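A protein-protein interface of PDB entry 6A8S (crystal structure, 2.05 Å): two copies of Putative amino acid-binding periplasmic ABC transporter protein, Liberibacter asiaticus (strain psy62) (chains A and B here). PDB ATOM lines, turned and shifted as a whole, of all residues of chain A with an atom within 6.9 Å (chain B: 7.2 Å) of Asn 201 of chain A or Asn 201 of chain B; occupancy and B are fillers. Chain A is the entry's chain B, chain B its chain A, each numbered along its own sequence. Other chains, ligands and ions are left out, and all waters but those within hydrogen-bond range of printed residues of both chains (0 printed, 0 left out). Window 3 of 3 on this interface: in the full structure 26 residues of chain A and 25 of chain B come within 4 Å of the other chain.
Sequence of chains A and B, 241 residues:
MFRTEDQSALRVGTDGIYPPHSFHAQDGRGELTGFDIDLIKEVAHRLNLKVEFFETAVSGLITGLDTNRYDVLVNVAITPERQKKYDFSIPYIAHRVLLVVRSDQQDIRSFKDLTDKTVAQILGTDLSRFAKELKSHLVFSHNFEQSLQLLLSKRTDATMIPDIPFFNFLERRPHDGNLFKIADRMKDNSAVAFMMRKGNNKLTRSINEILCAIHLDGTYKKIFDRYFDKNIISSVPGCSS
The guanidinium group (NH1) of Arg 205 of chain B is in hydrogen-bond range of the side-chain amide oxygen (OD1) of Asn 201 of chain A (3.4 Å).
The side-chain amide nitrogen of Asn 201 of chain A is in hydrogen-bond range of the side-chain amide oxygen of Asn 201 of chain B.
NH2 of Arg 205 of chain A sits close to N of Gly 199 of chain B (3.5 Å).
ND2 of Asn 201 of chain B lies close to NH2 of Arg 205 of chain A (3.2 Å).
The side-chain carboxylate (OD1) of Asp 87 of chain A lies within salt-bridge range of the guanidinium group (NH1) of Arg 205 of chain B.
The guanidinium group (NE) of Arg 205 of chain A is in salt-bridge range of the side-chain carboxylate (OD1) of Asp 87 of chain B.
The side-chain carboxylate (OD2) of Asp 87 of chain A sits at hydrogen-bond distance from the backbone NH (N) of Asn 200 of chain A (3.1 Å).
The backbone carbonyl oxygen (O) of Gly 199 of chain A lies close to the side-chain amide oxygen (OD1) of Asn 201 of chain A.
OD2 of Asp 87 of chain B lies within hydrogen-bond range of N of Gly 199 of chain B (3.1 Å).
The backbone carbonyl oxygen (O) of Gly 199 of chain B sits close to the side-chain amide oxygen (OD1) of Asn 201 of chain B.
The backbone carbonyl oxygen (O) of Asn 201 of chain A lies close to the guanidinium group (NH1) of Arg 205 of chain A (3.5 Å).
The side-chain carboxylate (OD2) of Asp 87 of chain A lies close to the side-chain amide oxygen (OD1) of Asn 201 of chain A, 3.3 Å away.
NH1 of Arg 205 of chain B touches N of Gly 199 of chain A, at 3.8 Å.
Lys 198 of chain A touches none of the printed residues of chain B.
Of the printed residues of chain B, Gly 199 of chain A touches Arg 205 (3.8 Å).
Of the printed residues of chain B, Asn 201 of chain A touches Asn 201 (2.9 Å) and Arg 205 (3.4 Å).
Lys 198 of chain B touches none of the printed residues of chain A.
Of the printed residues of chain A, Gly 199 of chain B touches Arg 205 (3.5 Å).
Printed residues of chain A within 4 Å of Asn 201 of chain B: Asn 201 and Arg 205.
Of the printed residues of chain A, Arg 205 of chain B touches Asp 87 (2.8 Å), Gly 199 (3.8 Å) and Asn 201 (3.4 Å).
Of the 11 printed residues of chain A, 4 touch a printed residue of chain B.
Printed residues of chain A that touch a printed residue of chain B: Asp 87, Gly 199, Asn 201 and Arg 205.
Of the 13 printed residues of chain B, 4 touch a printed residue of chain A.
Among the printed residues, 7 pairs touch across the chains.
Among the printed residues, Asp or Glu carboxylates within 4 Å of a Lys or Arg side-chain nitrogen of the other chain: Asp 87 of chain A with Arg 205 of chain B and Arg 205 of chain A with Asp 87 of chain B.
Asp 87 of chain A touches Arg 205 of chain B, and with the chains exchanged Arg 205 of chain A touches Asp 87 of chain B.
Gly 199 of chain A touches Arg 205 of chain B, and with the chains exchanged Arg 205 of chain A touches Gly 199 of chain B.
Asn 201 of chain A touches its own counterpart, Asn 201 of chain B.
Asn 201 of chain A touches Arg 205 of chain B, and with the chains exchanged Arg 205 of chain A touches Asn 201 of chain B.
Positions printed for both chains: 87, 197, 198, 199, 200, 201, 202, 203, 204, 205 and 206.
Of the 7 pairs that touch across the chains among the printed residues, 7 have their exchanged pair printed and touching as well.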
ATOM      1  N   ASP A  87       7.105 -13.798 -26.702  1.00  0.00           N
ATOM      2  CA  ASP A  87       8.298 -13.516 -25.914  1.00  0.00           C
ATOM      3  C   ASP A  87       9.118 -14.795 -25.743  1.00  0.00           C
ATOM      4  O   ASP A  87       8.560 -15.875 -25.534  1.00  0.00           O
ATOM      5  CB  ASP A  87       7.915 -12.977 -24.537  1.00  0.00           C
ATOM      6  CG  ASP A  87       7.602 -11.488 -24.547  1.00  0.00           C
ATOM      7  OD1 ASP A  87       8.048 -10.782 -25.476  1.00  0.00           O
ATOM      8  OD2 ASP A  87       6.924 -11.032 -23.605  1.00  0.00           O
ATOM      9  N   ARG A 197       3.709 -15.772 -23.739  1.00  0.00           N
ATOM     10  CA  ARG A 197       2.850 -14.786 -24.382  1.00  0.00           C
ATOM     11  C   ARG A 197       3.599 -13.475 -24.556  1.00  0.00           C
ATOM     12  O   ARG A 197       4.431 -13.100 -23.722  1.00  0.00           O
ATOM     13  CB  ARG A 197       1.597 -14.522 -23.548  1.00  0.00           C
ATOM     14  CG  ARG A 197       0.538 -15.597 -23.576  1.00  0.00           C
ATOM     15  CD  ARG A 197      -0.599 -15.200 -22.635  1.00  0.00           C
ATOM     16  NE  ARG A 197      -1.217 -13.928 -23.011  1.00  0.00           N
ATOM     17  CZ  ARG A 197      -1.115 -12.791 -22.321  1.00  0.00           C
ATOM     18  NH1 ARG A 197      -1.732 -11.699 -22.756  1.00  0.00           N
ATOM     19  NH2 ARG A 197      -0.403 -12.738 -21.202  1.00  0.00           N
ATOM     20  N   LYS A 198       3.293 -12.769 -25.645  1.00  0.00           N
ATOM     21  CA  LYS A 198       3.916 -11.479 -25.868  1.00  0.00           C
ATOM     22  C   LYS A 198       3.486 -10.500 -24.790  1.00  0.00           C
ATOM     23  O   LYS A 198       2.306 -10.426 -24.440  1.00  0.00           O
ATOM     24  CB  LYS A 198       3.535 -10.953 -27.248  1.00  0.00           C
ATOM     25  CG  LYS A 198       4.130  -9.600 -27.569  1.00  0.00           C
ATOM     26  CD  LYS A 198       3.226  -8.817 -28.496  1.00  0.00           C
ATOM     27  CE  LYS A 198       3.871  -8.583 -29.844  1.00  0.00           C
ATOM     28  NZ  LYS A 198       3.536  -7.224 -30.374  1.00  0.00           N
ATOM     29  N   GLY A 199       4.449  -9.766 -24.248  1.00  0.00           N
ATOM     30  CA  GLY A 199       4.176  -8.789 -23.216  1.00  0.00           C
ATOM     31  C   GLY A 199       4.383  -9.287 -21.803  1.00  0.00           C
ATOM     32  O   GLY A 199       4.365  -8.472 -20.872  1.00  0.00           O
ATOM     33  N   ASN A 200       4.593 -10.596 -21.619  1.00  0.00           N
ATOM     34  CA  ASN A 200       4.900 -11.187 -20.320  1.00  0.00           C
ATOM     35  C   ASN A 200       6.347 -10.882 -19.943  1.00  0.00           C
ATOM     36  O   ASN A 200       7.124 -11.788 -19.621  1.00  0.00           O
ATOM     37  CB  ASN A 200       4.644 -12.701 -20.362  1.00  0.00           C
ATOM     38  CG  ASN A 200       4.032 -13.234 -19.079  1.00  0.00           C
ATOM     39  OD1 ASN A 200       4.293 -12.721 -17.988  1.00  0.00           O
ATOM     40  ND2 ASN A 200       3.200 -14.269 -19.207  1.00  0.00           N
ATOM     41  N   ASN A 201       6.707  -9.596 -19.970  1.00  0.00           N
ATOM     42  CA  ASN A 201       8.108  -9.196 -19.887  1.00  0.00           C
ATOM     43  C   ASN A 201       8.711  -9.492 -18.526  1.00  0.00           C
ATOM     44  O   ASN A 201       9.919  -9.716 -18.420  1.00  0.00           O
ATOM     45  CB  ASN A 201       8.238  -7.707 -20.201  1.00  0.00           C
ATOM     46  CG  ASN A 201       7.305  -7.273 -21.300  1.00  0.00           C
ATOM     47  OD1 ASN A 201       7.099  -8.002 -22.275  1.00  0.00           O
ATOM     48  ND2 ASN A 201       6.727  -6.086 -21.154  1.00  0.00           N
ATOM     49  N   LYS A 202       7.900  -9.493 -17.483  1.00  0.00           N
ATOM     50  CA  LYS A 202       8.431  -9.646 -16.141  1.00  0.00           C
ATOM     51  C   LYS A 202       8.759 -11.107 -15.837  1.00  0.00           C
ATOM     52  O   LYS A 202       9.800 -11.394 -15.237  1.00  0.00           O
ATOM     53  CB  LYS A 202       7.431  -9.070 -15.138  1.00  0.00           C
ATOM     54  CG  LYS A 202       6.826  -7.666 -15.502  1.00  0.00           C
ATOM     55  CD  LYS A 202       5.802  -7.664 -16.681  1.00  0.00           C
ATOM     56  CE  LYS A 202       4.514  -8.407 -16.350  1.00  0.00           C
ATOM     57  NZ  LYS A 202       3.488  -8.286 -17.425  1.00  0.00           N
ATOM     58  N   LEU A 203       7.901 -12.040 -16.256  1.00  0.00           N
ATOM     59  CA  LEU A 203       8.257 -13.452 -16.173  1.00  0.00           C
ATOM     60  C   LEU A 203       9.484 -13.751 -17.022  1.00  0.00           C
ATOM     61  O   LEU A 203      10.361 -14.520 -16.613  1.00  0.00           O
ATOM     62  CB  LEU A 203       7.081 -14.326 -16.614  1.00  0.00           C
ATOM     63  CG  LEU A 203       7.421 -15.809 -16.773  1.00  0.00           C
ATOM     64  CD1 LEU A 203       7.742 -16.445 -15.442  1.00  0.00           C
ATOM     65  CD2 LEU A 203       6.297 -16.529 -17.451  1.00  0.00           C
ATOM     66  N   THR A 204       9.574 -13.127 -18.198  1.00  0.00           N
ATOM     67  CA  THR A 204      10.701 -13.382 -19.096  1.00  0.00           C
ATOM     68  C   THR A 204      12.022 -12.966 -18.462  1.00  0.00           C
ATOM     69  O   THR A 204      13.007 -13.711 -18.506  1.00  0.00           O
ATOM     70  CB  THR A 204      10.489 -12.648 -20.420  1.00  0.00           C
ATOM     71  OG1 THR A 204       9.349 -13.202 -21.079  1.00  0.00           O
ATOM     72  CG2 THR A 204      11.718 -12.805 -21.326  1.00  0.00           C
ATOM     73  N   ARG A 205      12.060 -11.765 -17.877  1.00  0.00           N
ATOM     74  CA  ARG A 205      13.262 -11.301 -17.194  1.00  0.00           C
ATOM     75  C   ARG A 205      13.630 -12.221 -16.035  1.00  0.00           C
ATOM     76  O   ARG A 205      14.807 -12.542 -15.835  1.00  0.00           O
ATOM     77  CB  ARG A 205      13.056  -9.870 -16.688  1.00  0.00           C
ATOM     78  CG  ARG A 205      12.948  -8.810 -17.776  1.00  0.00           C
ATOM     79  CD  ARG A 205      13.017  -7.403 -17.165  1.00  0.00           C
ATOM     80  NE  ARG A 205      12.910  -6.341 -18.162  1.00  0.00           N
ATOM     81  CZ  ARG A 205      11.762  -5.834 -18.602  1.00  0.00           C
ATOM     82  NH1 ARG A 205      10.602  -6.296 -18.145  1.00  0.00           N
ATOM     83  NH2 ARG A 205      11.774  -4.862 -19.505  1.00  0.00           N
ATOM     84  N   SER A 206      12.635 -12.649 -15.255  1.00  0.00           N
ATOM     85  CA  SER A 206      12.903 -13.523 -14.118  1.00  0.00           C
ATOM     86  C   SER A 206      13.537 -14.828 -14.578  1.00  0.00           C
ATOM     87  O   SER A 206      14.544 -15.279 -14.020  1.00  0.00           O
ATOM     88  CB  SER A 206      11.605 -13.799 -13.363  1.00  0.00           C
ATOM     89  OG  SER A 206      10.850 -12.612 -13.220  1.00  0.00           O
ATOM     90  N   ASP B  87      17.610  -4.241 -19.967  1.00  0.00           N
ATOM     91  CA  ASP B  87      17.164  -5.211 -20.958  1.00  0.00           C
ATOM     92  C   ASP B  87      18.344  -5.628 -21.837  1.00  0.00           C
ATOM     93  O   ASP B  87      19.265  -4.849 -22.081  1.00  0.00           O
ATOM     94  CB  ASP B  87      16.046  -4.637 -21.829  1.00  0.00           C
ATOM     95  CG  ASP B  87      14.670  -4.732 -21.172  1.00  0.00           C
ATOM     96  OD1 ASP B  87      14.442  -5.644 -20.352  1.00  0.00           O
ATOM     97  OD2 ASP B  87      13.816  -3.881 -21.475  1.00  0.00           O
ATOM     98  N   ARG B 197      18.077   0.247 -21.727  1.00  0.00           N
ATOM     99  CA  ARG B 197      17.322   0.578 -20.529  1.00  0.00           C
ATOM    100  C   ARG B 197      16.115  -0.349 -20.405  1.00  0.00           C
ATOM    101  O   ARG B 197      15.544  -0.792 -21.401  1.00  0.00           O
ATOM    102  CB  ARG B 197      16.864   2.041 -20.575  1.00  0.00           C
ATOM    103  CG  ARG B 197      17.929   3.046 -20.152  1.00  0.00           C
ATOM    104  CD  ARG B 197      17.380   4.482 -20.238  1.00  0.00           C
ATOM    105  NE  ARG B 197      16.573   4.672 -21.437  1.00  0.00           N
ATOM    106  CZ  ARG B 197      17.057   5.052 -22.616  1.00  0.00           C
ATOM    107  NH1 ARG B 197      18.350   5.294 -22.746  1.00  0.00           N
ATOM    108  NH2 ARG B 197      16.249   5.183 -23.667  1.00  0.00           N
ATOM    109  N   LYS B 198      15.748  -0.675 -19.167  1.00  0.00           N
ATOM    110  CA  LYS B 198      14.549  -1.481 -18.955  1.00  0.00           C
ATOM    111  C   LYS B 198      13.327  -0.743 -19.474  1.00  0.00           C
ATOM    112  O   LYS B 198      13.245   0.480 -19.380  1.00  0.00           O
ATOM    113  CB  LYS B 198      14.368  -1.792 -17.473  1.00  0.00           C
ATOM    114  CG  LYS B 198      15.085  -3.027 -17.000  1.00  0.00           C
ATOM    115  CD  LYS B 198      14.971  -3.168 -15.493  1.00  0.00           C
ATOM    116  CE  LYS B 198      13.531  -3.391 -15.076  1.00  0.00           C
ATOM    117  NZ  LYS B 198      13.455  -4.266 -13.877  1.00  0.00           N
ATOM    118  N   GLY B 199      12.377  -1.486 -20.036  1.00  0.00           N
ATOM    119  CA  GLY B 199      11.118  -0.870 -20.396  1.00  0.00           C
ATOM    120  C   GLY B 199      10.645  -1.097 -21.813  1.00  0.00           C
ATOM    121  O   GLY B 199       9.582  -1.689 -22.030  1.00  0.00           O
ATOM    122  N   ASN B 200      11.413  -0.631 -22.796  1.00  0.00           N
ATOM    123  CA  ASN B 200      11.012  -0.764 -24.194  1.00  0.00           C
ATOM    124  C   ASN B 200      11.287  -2.193 -24.659  1.00  0.00           C
ATOM    125  O   ASN B 200      12.320  -2.515 -25.258  1.00  0.00           O
ATOM    126  CB  ASN B 200      11.720   0.256 -25.071  1.00  0.00           C
ATOM    127  CG  ASN B 200      11.187   0.252 -26.479  1.00  0.00           C
ATOM    128  OD1 ASN B 200      10.175  -0.385 -26.755  1.00  0.00           O
ATOM    129  ND2 ASN B 200      11.859   0.956 -27.380  1.00  0.00           N
ATOM    130  N   ASN B 201      10.328  -3.067 -24.367  1.00  0.00           N
ATOM    131  CA  ASN B 201      10.381  -4.415 -24.912  1.00  0.00           C
ATOM    132  C   ASN B 201      10.287  -4.405 -26.429  1.00  0.00           C
ATOM    133  O   ASN B 201      10.863  -5.277 -27.093  1.00  0.00           O
ATOM    134  CB  ASN B 201       9.252  -5.239 -24.310  1.00  0.00           C
ATOM    135  CG  ASN B 201       8.978  -4.853 -22.887  1.00  0.00           C
ATOM    136  OD1 ASN B 201       8.104  -4.030 -22.608  1.00  0.00           O
ATOM    137  ND2 ASN B 201       9.749  -5.421 -21.968  1.00  0.00           N
ATOM    138  N   LYS B 202       9.577  -3.426 -26.993  1.00  0.00           N
ATOM    139  CA  LYS B 202       9.342  -3.418 -28.430  1.00  0.00           C
ATOM    140  C   LYS B 202      10.651  -3.377 -29.202  1.00  0.00           C
ATOM    141  O   LYS B 202      10.839  -4.126 -30.167  1.00  0.00           O
ATOM    142  CB  LYS B 202       8.444  -2.242 -28.822  1.00  0.00           C
ATOM    143  CG  LYS B 202       7.497  -2.569 -29.982  1.00  0.00           C
ATOM    144  CD  LYS B 202       6.505  -1.445 -30.275  1.00  0.00           C
ATOM    145  CE  LYS B 202       5.287  -1.525 -29.364  1.00  0.00           C
ATOM    146  NZ  LYS B 202       4.521  -0.243 -29.318  1.00  0.00           N
ATOM    147  N   LEU B 203      11.578  -2.514 -28.790  1.00  0.00           N
ATOM    148  CA  LEU B 203      12.840  -2.432 -29.511  1.00  0.00           C
ATOM    149  C   LEU B 203      13.679  -3.684 -29.288  1.00  0.00           C
ATOM    150  O   LEU B 203      14.367  -4.143 -30.205  1.00  0.00           O
ATOM    151  CB  LEU B 203      13.612  -1.179 -29.105  1.00  0.00           C
ATOM    152  CG  LEU B 203      15.032  -1.092 -29.666  1.00  0.00           C
ATOM    153  CD1 LEU B 203      14.992  -0.613 -31.103  1.00  0.00           C
ATOM    154  CD2 LEU B 203      15.898  -0.165 -28.838  1.00  0.00           C
ATOM    155  N   THR B 204      13.639  -4.248 -28.080  1.00  0.00           N
ATOM    156  CA  THR B 204      14.373  -5.484 -27.821  1.00  0.00           C
ATOM    157  C   THR B 204      13.886  -6.611 -28.728  1.00  0.00           C
ATOM    158  O   THR B 204      14.690  -7.293 -29.377  1.00  0.00           O
ATOM    159  CB  THR B 204      14.233  -5.868 -26.350  1.00  0.00           C
ATOM    160  OG1 THR B 204      14.878  -4.880 -25.547  1.00  0.00           O
ATOM    161  CG2 THR B 204      14.866  -7.209 -26.082  1.00  0.00           C
ATOM    162  N   ARG B 205      12.565  -6.824 -28.775  1.00  0.00           N
ATOM    163  CA  ARG B 205      12.006  -7.879 -29.619  1.00  0.00           C
ATOM    164  C   ARG B 205      12.374  -7.671 -31.086  1.00  0.00           C
ATOM    165  O   ARG B 205      12.758  -8.621 -31.783  1.00  0.00           O
ATOM    166  CB  ARG B 205      10.482  -7.938 -29.449  1.00  0.00           C
ATOM    167  CG  ARG B 205       9.999  -8.659 -28.187  1.00  0.00           C
ATOM    168  CD  ARG B 205       8.475  -8.863 -28.193  1.00  0.00           C
ATOM    169  NE  ARG B 205       7.757  -7.621 -27.926  1.00  0.00           N
ATOM    170  CZ  ARG B 205       7.327  -7.242 -26.726  1.00  0.00           C
ATOM    171  NH1 ARG B 205       7.530  -8.011 -25.670  1.00  0.00           N
ATOM    172  NH2 ARG B 205       6.688  -6.087 -26.582  1.00  0.00           N
ATOM    173  N   SER B 206      12.265  -6.431 -31.571  1.00  0.00           N
ATOM    174  CA  SER B 206      12.584  -6.148 -32.967  1.00  0.00           C
ATOM    175  C   SER B 206      14.055  -6.419 -33.265  1.00  0.00           C
ATOM    176  O   SER B 206      14.391  -6.968 -34.319  1.00  0.00           O
ATOM    177  CB  SER B 206      12.233  -4.699 -33.302  1.00  0.00           C
ATOM    178  OG  SER B 206      10.843  -4.471 -33.162  1.00  0.00           O
ATOM    179  N   ILE B 207      14.948  -6.027 -32.356  1.00  0.00           N
ATOM    180  CA  ILE B 207      16.360  -6.357 -32.531  1.00  0.00           C
ATOM    181  C   ILE B 207      16.538  -7.871 -32.582  1.00  0.00           C
ATOM    182  O   ILE B 207      17.214  -8.399 -33.471  1.00  0.00           O
ATOM    183  CB  ILE B 207      17.207  -5.715 -31.420  1.00  0.00           C
ATOM    184  CG1 ILE B 207      17.152  -4.181 -31.520  1.00  0.00           C
ATOM    185  CG2 ILE B 207      18.639  -6.238 -31.463  1.00  0.00           C
ATOM    186  CD1 ILE B 207      17.909  -3.463 -30.413  1.00  0.00           C
ATOM    187  N   ASN B 208      15.921  -8.590 -31.639  1.00  0.00           N
ATOM    188  CA  ASN B 208      16.051 -10.049 -31.613  1.00  0.00           C
ATOM    189  C   ASN B 208      15.541 -10.678 -32.892  1.00  0.00           C
ATOM    190  O   ASN B 208      16.097 -11.676 -33.371  1.00  0.00           O
ATOM    191  CB  ASN B 208      15.293 -10.645 -30.430  1.00  0.00           C
ATOM    192  CG  ASN B 208      15.926 -10.314 -29.128  1.00  0.00           C
ATOM    193  OD1 ASN B 208      17.033  -9.778 -29.091  1.00  0.00           O
ATOM    194  ND2 ASN B 208      15.233 -10.623 -28.038  1.00  0.00           N
